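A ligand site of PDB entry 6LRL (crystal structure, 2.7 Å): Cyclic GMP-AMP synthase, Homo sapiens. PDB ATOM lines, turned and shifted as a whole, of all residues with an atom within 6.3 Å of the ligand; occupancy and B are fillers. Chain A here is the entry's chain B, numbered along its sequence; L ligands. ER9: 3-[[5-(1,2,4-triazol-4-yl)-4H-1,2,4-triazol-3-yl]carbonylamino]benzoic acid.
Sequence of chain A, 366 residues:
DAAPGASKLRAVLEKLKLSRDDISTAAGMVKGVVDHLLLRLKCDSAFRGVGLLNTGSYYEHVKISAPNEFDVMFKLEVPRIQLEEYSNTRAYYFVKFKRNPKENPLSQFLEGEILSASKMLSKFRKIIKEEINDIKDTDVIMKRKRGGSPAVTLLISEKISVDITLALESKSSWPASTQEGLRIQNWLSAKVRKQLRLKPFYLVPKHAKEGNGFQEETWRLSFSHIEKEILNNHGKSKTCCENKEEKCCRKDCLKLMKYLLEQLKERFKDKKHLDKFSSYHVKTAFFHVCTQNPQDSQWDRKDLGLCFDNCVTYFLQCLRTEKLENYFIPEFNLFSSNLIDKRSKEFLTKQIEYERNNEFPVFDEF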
ATOM      1  N   ALA A  91       1.551  33.354 -24.720  1.00  0.00           N
ATOM      2  CA  ALA A  91       0.629  32.730 -23.783  1.00  0.00           C
ATOM      3  C   ALA A  91       1.321  31.959 -22.675  1.00  0.00           C
ATOM      4  O   ALA A  91       0.647  31.607 -21.705  1.00  0.00           O
ATOM      5  CB  ALA A  91      -0.332  31.790 -24.522  1.00  0.00           C
ATOM      6  N   TYR A  92       2.611  31.682 -22.772  1.00  0.00           N
ATOM      7  CA  TYR A  92       3.368  31.000 -21.734  1.00  0.00           C
ATOM      8  C   TYR A  92       4.418  31.947 -21.188  1.00  0.00           C
ATOM      9  O   TYR A  92       5.048  32.697 -21.955  1.00  0.00           O
ATOM     10  CB  TYR A  92       4.017  29.719 -22.270  1.00  0.00           C
ATOM     11  CG  TYR A  92       3.020  28.697 -22.778  1.00  0.00           C
ATOM     12  CD1 TYR A  92       2.364  28.877 -23.989  1.00  0.00           C
ATOM     13  CD2 TYR A  92       2.728  27.551 -22.044  1.00  0.00           C
ATOM     14  CE1 TYR A  92       1.453  27.946 -24.453  1.00  0.00           C
ATOM     15  CE2 TYR A  92       1.817  26.621 -22.507  1.00  0.00           C
ATOM     16  CZ  TYR A  92       1.185  26.825 -23.710  1.00  0.00           C
ATOM     17  OH  TYR A  92       0.280  25.898 -24.179  1.00  0.00           O
ATOM     18  N   ARG A 220       0.880  29.236 -18.241  1.00  0.00           N
ATOM     19  CA  ARG A 220       0.010  29.757 -19.296  1.00  0.00           C
ATOM     20  C   ARG A 220      -1.103  30.607 -18.712  1.00  0.00           C
ATOM     21  O   ARG A 220      -1.592  30.341 -17.611  1.00  0.00           O
ATOM     22  CB  ARG A 220      -0.589  28.617 -20.128  1.00  0.00           C
ATOM     23  CG  ARG A 220      -1.404  29.126 -21.309  1.00  0.00           C
ATOM     24  CD  ARG A 220      -2.038  28.005 -22.122  1.00  0.00           C
ATOM     25  NE  ARG A 220      -2.845  27.112 -21.304  1.00  0.00           N
ATOM     26  CZ  ARG A 220      -3.069  25.836 -21.601  1.00  0.00           C
ATOM     27  NH1 ARG A 220      -2.551  25.325 -22.705  1.00  0.00           N
ATOM     28  NH2 ARG A 220      -3.813  25.093 -20.804  1.00  0.00           N
ATOM     29  N   LEU A 221      -1.499  31.633 -19.460  1.00  0.00           N
ATOM     30  CA  LEU A 221      -2.629  32.464 -19.101  1.00  0.00           C
ATOM     31  C   LEU A 221      -3.876  31.610 -18.891  1.00  0.00           C
ATOM     32  O   LEU A 221      -4.077  30.598 -19.570  1.00  0.00           O
ATOM     33  CB  LEU A 221      -2.897  33.492 -20.205  1.00  0.00           C
ATOM     34  CG  LEU A 221      -1.864  34.589 -20.454  1.00  0.00           C
ATOM     35  CD1 LEU A 221      -2.548  35.818 -20.999  1.00  0.00           C
ATOM     36  CD2 LEU A 221      -1.109  34.928 -19.183  1.00  0.00           C
ATOM     37  N   SER A 222      -4.710  32.022 -17.941  1.00  0.00           N
ATOM     38  CA  SER A 222      -5.987  31.375 -17.694  1.00  0.00           C
ATOM     39  C   SER A 222      -6.992  32.432 -17.281  1.00  0.00           C
ATOM     40  O   SER A 222      -6.711  33.241 -16.380  1.00  0.00           O
ATOM     41  CB  SER A 222      -5.877  30.288 -16.621  1.00  0.00           C
ATOM     42  OG  SER A 222      -7.093  29.570 -16.513  1.00  0.00           O
ATOM     43  N   PHE A 223      -8.146  32.427 -17.925  1.00  0.00           N
ATOM     44  CA  PHE A 223      -9.241  33.348 -17.623  1.00  0.00           C
ATOM     45  C   PHE A 223     -10.542  32.565 -17.438  1.00  0.00           C
ATOM     46  O   PHE A 223     -11.613  32.989 -17.889  1.00  0.00           O
ATOM     47  CB  PHE A 223      -9.388  34.408 -18.708  1.00  0.00           C
ATOM     48  CG  PHE A 223      -8.104  35.154 -18.988  1.00  0.00           C
ATOM     49  CD1 PHE A 223      -7.787  36.298 -18.272  1.00  0.00           C
ATOM     50  CD2 PHE A 223      -7.231  34.705 -19.964  1.00  0.00           C
ATOM     51  CE1 PHE A 223      -6.617  36.978 -18.530  1.00  0.00           C
ATOM     52  CE2 PHE A 223      -6.047  35.388 -20.220  1.00  0.00           C
ATOM     53  CZ  PHE A 223      -5.744  36.530 -19.506  1.00  0.00           C
ATOM     54  N   GLU A 227     -14.468  33.463 -18.183  1.00  0.00           N
ATOM     55  CA  GLU A 227     -15.310  32.646 -19.059  1.00  0.00           C
ATOM     56  C   GLU A 227     -16.649  32.345 -18.389  1.00  0.00           C
ATOM     57  O   GLU A 227     -17.712  32.503 -19.010  1.00  0.00           O
ATOM     58  CB  GLU A 227     -14.586  31.349 -19.423  1.00  0.00           C
ATOM     59  CG  GLU A 227     -13.595  31.485 -20.569  1.00  0.00           C
ATOM     60  CD  GLU A 227     -12.506  30.432 -20.527  1.00  0.00           C
ATOM     61  OE1 GLU A 227     -11.333  30.777 -20.777  1.00  0.00           O
ATOM     62  OE2 GLU A 227     -12.827  29.261 -20.244  1.00  0.00           O
ATOM     63  N   ASP A 275      -8.642  13.030 -30.328  1.00  0.00           N
ATOM     64  CA  ASP A 275      -8.289  13.127 -28.919  1.00  0.00           C
ATOM     65  C   ASP A 275      -7.542  14.415 -28.587  1.00  0.00           C
ATOM     66  O   ASP A 275      -7.447  14.771 -27.402  1.00  0.00           O
ATOM     67  CB  ASP A 275      -7.444  11.912 -28.507  1.00  0.00           C
ATOM     68  CG  ASP A 275      -6.415  11.532 -29.553  1.00  0.00           C
ATOM     69  OD1 ASP A 275      -6.494  12.063 -30.681  1.00  0.00           O
ATOM     70  OD2 ASP A 275      -5.521  10.713 -29.238  1.00  0.00           O
ATOM     71  N   LYS A 276      -7.015  15.109 -29.589  1.00  0.00           N
ATOM     72  CA  LYS A 276      -6.364  16.393 -29.347  1.00  0.00           C
ATOM     73  C   LYS A 276      -7.362  17.541 -29.284  1.00  0.00           C
ATOM     74  O   LYS A 276      -7.012  18.623 -28.788  1.00  0.00           O
ATOM     75  CB  LYS A 276      -5.327  16.676 -30.449  1.00  0.00           C
ATOM     76  N   PHE A 277      -8.581  17.341 -29.766  1.00  0.00           N
ATOM     77  CA  PHE A 277      -9.623  18.346 -29.656  1.00  0.00           C
ATOM     78  C   PHE A 277     -10.266  18.277 -28.269  1.00  0.00           C
ATOM     79  O   PHE A 277     -10.413  17.202 -27.688  1.00  0.00           O
ATOM     80  CB  PHE A 277     -10.686  18.167 -30.740  1.00  0.00           C
ATOM     81  CG  PHE A 277     -10.150  18.310 -32.133  1.00  0.00           C
ATOM     82  CD1 PHE A 277      -9.934  19.574 -32.684  1.00  0.00           C
ATOM     83  CD2 PHE A 277      -9.863  17.203 -32.906  1.00  0.00           C
ATOM     84  CE1 PHE A 277      -9.442  19.714 -33.961  1.00  0.00           C
ATOM     85  CE2 PHE A 277      -9.369  17.333 -34.186  1.00  0.00           C
ATOM     86  CZ  PHE A 277      -9.161  18.589 -34.718  1.00  0.00           C
ATOM     87  N   SER A 278     -10.644  19.434 -27.755  1.00  0.00           N
ATOM     88  CA  SER A 278     -11.203  19.525 -26.406  1.00  0.00           C
ATOM     89  C   SER A 278     -12.359  20.515 -26.399  1.00  0.00           C
ATOM     90  O   SER A 278     -12.505  21.353 -27.289  1.00  0.00           O
ATOM     91  CB  SER A 278     -10.139  19.939 -25.386  1.00  0.00           C
ATOM     92  OG  SER A 278     -10.702  20.705 -24.343  1.00  0.00           O
ATOM     93  N   SER A 279     -13.175  20.405 -25.344  1.00  0.00           N
ATOM     94  CA  SER A 279     -14.324  21.285 -25.187  1.00  0.00           C
ATOM     95  C   SER A 279     -13.920  22.754 -25.096  1.00  0.00           C
ATOM     96  O   SER A 279     -14.767  23.633 -25.298  1.00  0.00           O
ATOM     97  CB  SER A 279     -15.120  20.895 -23.947  1.00  0.00           C
ATOM     98  OG  SER A 279     -14.271  20.715 -22.833  1.00  0.00           O
ATOM     99  N   TYR A 280     -12.649  23.047 -24.803  1.00  0.00           N
ATOM    100  CA  TYR A 280     -12.215  24.430 -24.761  1.00  0.00           C
ATOM    101  C   TYR A 280     -12.149  25.037 -26.160  1.00  0.00           C
ATOM    102  O   TYR A 280     -12.289  26.255 -26.311  1.00  0.00           O
ATOM    103  CB  TYR A 280     -10.867  24.562 -24.068  1.00  0.00           C
ATOM    104  CG  TYR A 280     -10.510  26.009 -23.809  1.00  0.00           C
ATOM    105  CD1 TYR A 280     -11.195  26.739 -22.839  1.00  0.00           C
ATOM    106  CD2 TYR A 280      -9.538  26.657 -24.547  1.00  0.00           C
ATOM    107  CE1 TYR A 280     -10.892  28.063 -22.602  1.00  0.00           C
ATOM    108  CE2 TYR A 280      -9.225  27.975 -24.319  1.00  0.00           C
ATOM    109  CZ  TYR A 280      -9.907  28.682 -23.342  1.00  0.00           C
ATOM    110  OH  TYR A 280      -9.608  29.998 -23.115  1.00  0.00           O
ATOM    111  N   HIS A 281     -11.938  24.208 -27.189  1.00  0.00           N
ATOM    112  CA  HIS A 281     -12.001  24.712 -28.558  1.00  0.00           C
ATOM    113  C   HIS A 281     -13.428  25.083 -28.925  1.00  0.00           C
ATOM    114  O   HIS A 281     -13.673  26.154 -29.505  1.00  0.00           O
ATOM    115  CB  HIS A 281     -11.441  23.675 -29.526  1.00  0.00           C
ATOM    116  CG  HIS A 281     -10.020  23.292 -29.261  1.00  0.00           C
ATOM    117  ND1 HIS A 281      -9.617  21.974 -29.146  1.00  0.00           N
ATOM    118  CD2 HIS A 281      -8.904  24.041 -29.096  1.00  0.00           C
ATOM    119  CE1 HIS A 281      -8.321  21.939 -28.916  1.00  0.00           C
ATOM    120  NE2 HIS A 281      -7.864  23.170 -28.885  1.00  0.00           N
ATOM    121  N   ASN A 326      -7.209  32.398 -29.502  1.00  0.00           N
ATOM    122  CA  ASN A 326      -7.624  32.464 -28.106  1.00  0.00           C
ATOM    123  C   ASN A 326      -8.458  33.706 -27.880  1.00  0.00           C
ATOM    124  O   ASN A 326      -8.112  34.802 -28.351  1.00  0.00           O
ATOM    125  CB  ASN A 326      -6.390  32.470 -27.202  1.00  0.00           C
ATOM    126  CG  ASN A 326      -6.739  32.251 -25.739  1.00  0.00           C
ATOM    127  OD1 ASN A 326      -7.094  33.179 -25.023  1.00  0.00           O
ATOM    128  ND2 ASN A 326      -6.634  31.005 -25.286  1.00  0.00           N
ATOM    129  N   PHE A 328      -8.857  35.562 -25.448  1.00  0.00           N
ATOM    130  CA  PHE A 328      -8.169  36.599 -24.704  1.00  0.00           C
ATOM    131  C   PHE A 328      -6.809  36.952 -25.281  1.00  0.00           C
ATOM    132  O   PHE A 328      -6.389  38.102 -25.190  1.00  0.00           O
ATOM    133  CB  PHE A 328      -8.019  36.183 -23.241  1.00  0.00           C
ATOM    134  CG  PHE A 328      -9.306  35.738 -22.592  1.00  0.00           C
ATOM    135  CD1 PHE A 328      -9.711  34.414 -22.665  1.00  0.00           C
ATOM    136  CD2 PHE A 328     -10.114  36.645 -21.931  1.00  0.00           C
ATOM    137  CE1 PHE A 328     -10.888  34.004 -22.078  1.00  0.00           C
ATOM    138  CE2 PHE A 328     -11.293  36.244 -21.341  1.00  0.00           C
ATOM    139  CZ  PHE A 328     -11.688  34.914 -21.423  1.00  0.00           C
ATOM    140  N   ILE A 329      -6.117  35.985 -25.866  1.00  0.00           N
ATOM    141  CA  ILE A 329      -4.834  36.226 -26.523  1.00  0.00           C
ATOM    142  C   ILE A 329      -5.009  36.014 -28.017  1.00  0.00           C
ATOM    143  O   ILE A 329      -4.778  34.895 -28.522  1.00  0.00           O
ATOM    144  CB  ILE A 329      -3.736  35.300 -25.960  1.00  0.00           C
ATOM    145  CG1 ILE A 329      -3.775  35.312 -24.428  1.00  0.00           C
ATOM    146  CG2 ILE A 329      -2.370  35.728 -26.467  1.00  0.00           C
ATOM    147  CD1 ILE A 329      -4.115  33.971 -23.823  1.00  0.00           C
ATOM    148  N   PHE A 332      -2.631  33.904 -30.191  1.00  0.00           N
ATOM    149  CA  PHE A 332      -2.430  32.510 -29.810  1.00  0.00           C
ATOM    150  C   PHE A 332      -3.469  31.680 -30.548  1.00  0.00           C
ATOM    151  O   PHE A 332      -4.639  31.645 -30.158  1.00  0.00           O
ATOM    152  CB  PHE A 332      -2.524  32.353 -28.293  1.00  0.00           C
ATOM    153  CG  PHE A 332      -2.353  30.931 -27.812  1.00  0.00           C
ATOM    154  CD1 PHE A 332      -1.583  30.017 -28.508  1.00  0.00           C
ATOM    155  CD2 PHE A 332      -2.955  30.518 -26.633  1.00  0.00           C
ATOM    156  CE1 PHE A 332      -1.431  28.719 -28.062  1.00  0.00           C
ATOM    157  CE2 PHE A 332      -2.811  29.217 -26.181  1.00  0.00           C
ATOM    158  CZ  PHE A 332      -2.042  28.317 -26.888  1.00  0.00           C
ATOM    159  N   LEU A 334      -5.069  28.328 -31.349  1.00  0.00           N
ATOM    160  CA  LEU A 334      -5.197  26.971 -30.846  1.00  0.00           C
ATOM    161  C   LEU A 334      -5.240  25.944 -31.974  1.00  0.00           C
ATOM    162  O   LEU A 334      -4.923  24.773 -31.742  1.00  0.00           O
ATOM    163  CB  LEU A 334      -6.442  26.840 -29.970  1.00  0.00           C
ATOM    164  CG  LEU A 334      -6.572  27.874 -28.852  1.00  0.00           C
ATOM    165  CD1 LEU A 334      -7.812  28.746 -29.040  1.00  0.00           C
ATOM    166  CD2 LEU A 334      -6.591  27.193 -27.489  1.00  0.00           C
ATOM    167  N   PHE A 335      -5.618  26.346 -33.182  1.00  0.00           N
ATOM    168  CA  PHE A 335      -5.720  25.454 -34.336  1.00  0.00           C
ATOM    169  C   PHE A 335      -4.495  25.555 -35.238  1.00  0.00           C
ATOM    170  O   PHE A 335      -4.619  25.538 -36.462  1.00  0.00           O
ATOM    171  CB  PHE A 335      -6.989  25.745 -35.122  1.00  0.00           C
ATOM    172  CG  PHE A 335      -8.204  25.061 -34.577  1.00  0.00           C
ATOM    173  CD1 PHE A 335      -8.110  24.230 -33.472  1.00  0.00           C
ATOM    174  CD2 PHE A 335      -9.450  25.245 -35.173  1.00  0.00           C
ATOM    175  CE1 PHE A 335      -9.233  23.591 -32.973  1.00  0.00           C
ATOM    176  CE2 PHE A 335     -10.567  24.605 -34.666  1.00  0.00           C
ATOM    177  CZ  PHE A 335     -10.467  23.787 -33.564  1.00  0.00           C
ATOM    178  N   LEU A 339       0.218  22.512 -33.215  1.00  0.00           N
ATOM    179  CA  LEU A 339      -0.619  21.872 -32.196  1.00  0.00           C
ATOM    180  C   LEU A 339      -1.378  20.704 -32.817  1.00  0.00           C
ATOM    181  O   LEU A 339      -1.049  19.531 -32.570  1.00  0.00           O
ATOM    182  CB  LEU A 339      -1.578  22.885 -31.577  1.00  0.00           C
HETATM  183  C4  ER9 L   1      -7.581  24.311 -21.758  1.00  0.00           C
HETATM  184  C5  ER9 L   1      -7.545  22.839 -21.826  1.00  0.00           C
HETATM  185  C6  ER9 L   1      -6.277  22.082 -23.816  1.00  0.00           C
HETATM  186  C11 ER9 L   1      -5.456  22.895 -24.578  1.00  0.00           C
HETATM  187  C7  ER9 L   1      -6.958  21.020 -24.411  1.00  0.00           C
HETATM  188  C8  ER9 L   1      -6.783  20.767 -25.760  1.00  0.00           C
HETATM  189  C9  ER9 L   1      -5.960  21.571 -26.524  1.00  0.00           C
HETATM  190  C10 ER9 L   1      -5.287  22.643 -25.934  1.00  0.00           C
HETATM  191  C12 ER9 L   1      -4.398  23.523 -26.758  1.00  0.00           C
HETATM  192  N1  ER9 L   1      -6.105  29.668 -22.877  1.00  0.00           N
HETATM  193  N2  ER9 L   1      -5.454  28.935 -23.858  1.00  0.00           N
HETATM  194  C3  ER9 L   1      -7.123  26.394 -22.110  1.00  0.00           C
HETATM  195  N3  ER9 L   1      -6.586  27.576 -22.612  1.00  0.00           N
HETATM  196  C1  ER9 L   1      -6.766  28.837 -22.147  1.00  0.00           C
HETATM  197  C2  ER9 L   1      -5.755  27.694 -23.679  1.00  0.00           C
HETATM  198  N4  ER9 L   1      -6.782  25.114 -22.502  1.00  0.00           N
HETATM  199  N5  ER9 L   1      -8.360  24.991 -20.938  1.00  0.00           N
HETATM  200  N6  ER9 L   1      -8.078  26.299 -21.171  1.00  0.00           N
HETATM  201  N7  ER9 L   1      -6.440  22.360 -22.436  1.00  0.00           N
HETATM  202  O1  ER9 L   1      -8.465  22.154 -21.373  1.00  0.00           O
HETATM  203  O2  ER9 L   1      -3.733  24.397 -26.159  1.00  0.00           O
HETATM  204  O3  ER9 L   1      -4.367  23.340 -27.989  1.00  0.00           O
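A nitrogen (N2) of the ligand is in hydrogen-bond range of the side-chain amide nitrogen (ND2) of Asn 326.
The guanidinium group (NH1) of Arg 220 lies within salt-bridge range of an oxygen (O2) of the ligand, at 3.8 Å.
The backbone NH (N) of Phe 328 lies within hydrogen-bond range of the side-chain amide oxygen (OD1) of Asn 326, at 3.0 Å.
NH1 of Arg 220 lies within hydrogen-bond range of OH of Tyr 92, at 3.2 Å.
The side-chain hydroxyl (OG) of Ser 278 sits close to the backbone NH (N) of Tyr 280 (3.1 Å).
OD1 of Asn 326 lies within hydrogen-bond range of N of Ile 329 (3.1 Å).
O of Ala 91 lies within hydrogen-bond range of N of Leu 221, at 3.1 Å.
ND1 of His 281 is in hydrogen-bond range of N of Ser 278 (3.1 Å).
O of Phe 332 sits at hydrogen-bond distance from N of Asn 326 (2.8 Å).
OE1 of Glu 227 sits at hydrogen-bond distance from OH of Tyr 280, 3.0 Å away.
Merely in contact with the ligand: Leu 221 (3.99 Å), Lys 276 (3.7 Å), Ser 278 (3.5 Å), Tyr 280 (3.2 Å), His 281 (3.4 Å), Phe 332 (3.5 Å) and Leu 334 (3.9 Å).
Hydrophobic or aromatic side chains within 4 Å of the ligand: Tyr 280, His 281, Phe 332 and Leu 334.
Nine residues have an atom within 4 Å of the ligand: Arg 220, Leu 221, Lys 276, Ser 278, Tyr 280, His 281, Asn 326, Phe 332 and Leu 334.
The nearest printed residue that does not touch the ligand is Leu 339 (4.6 Å).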
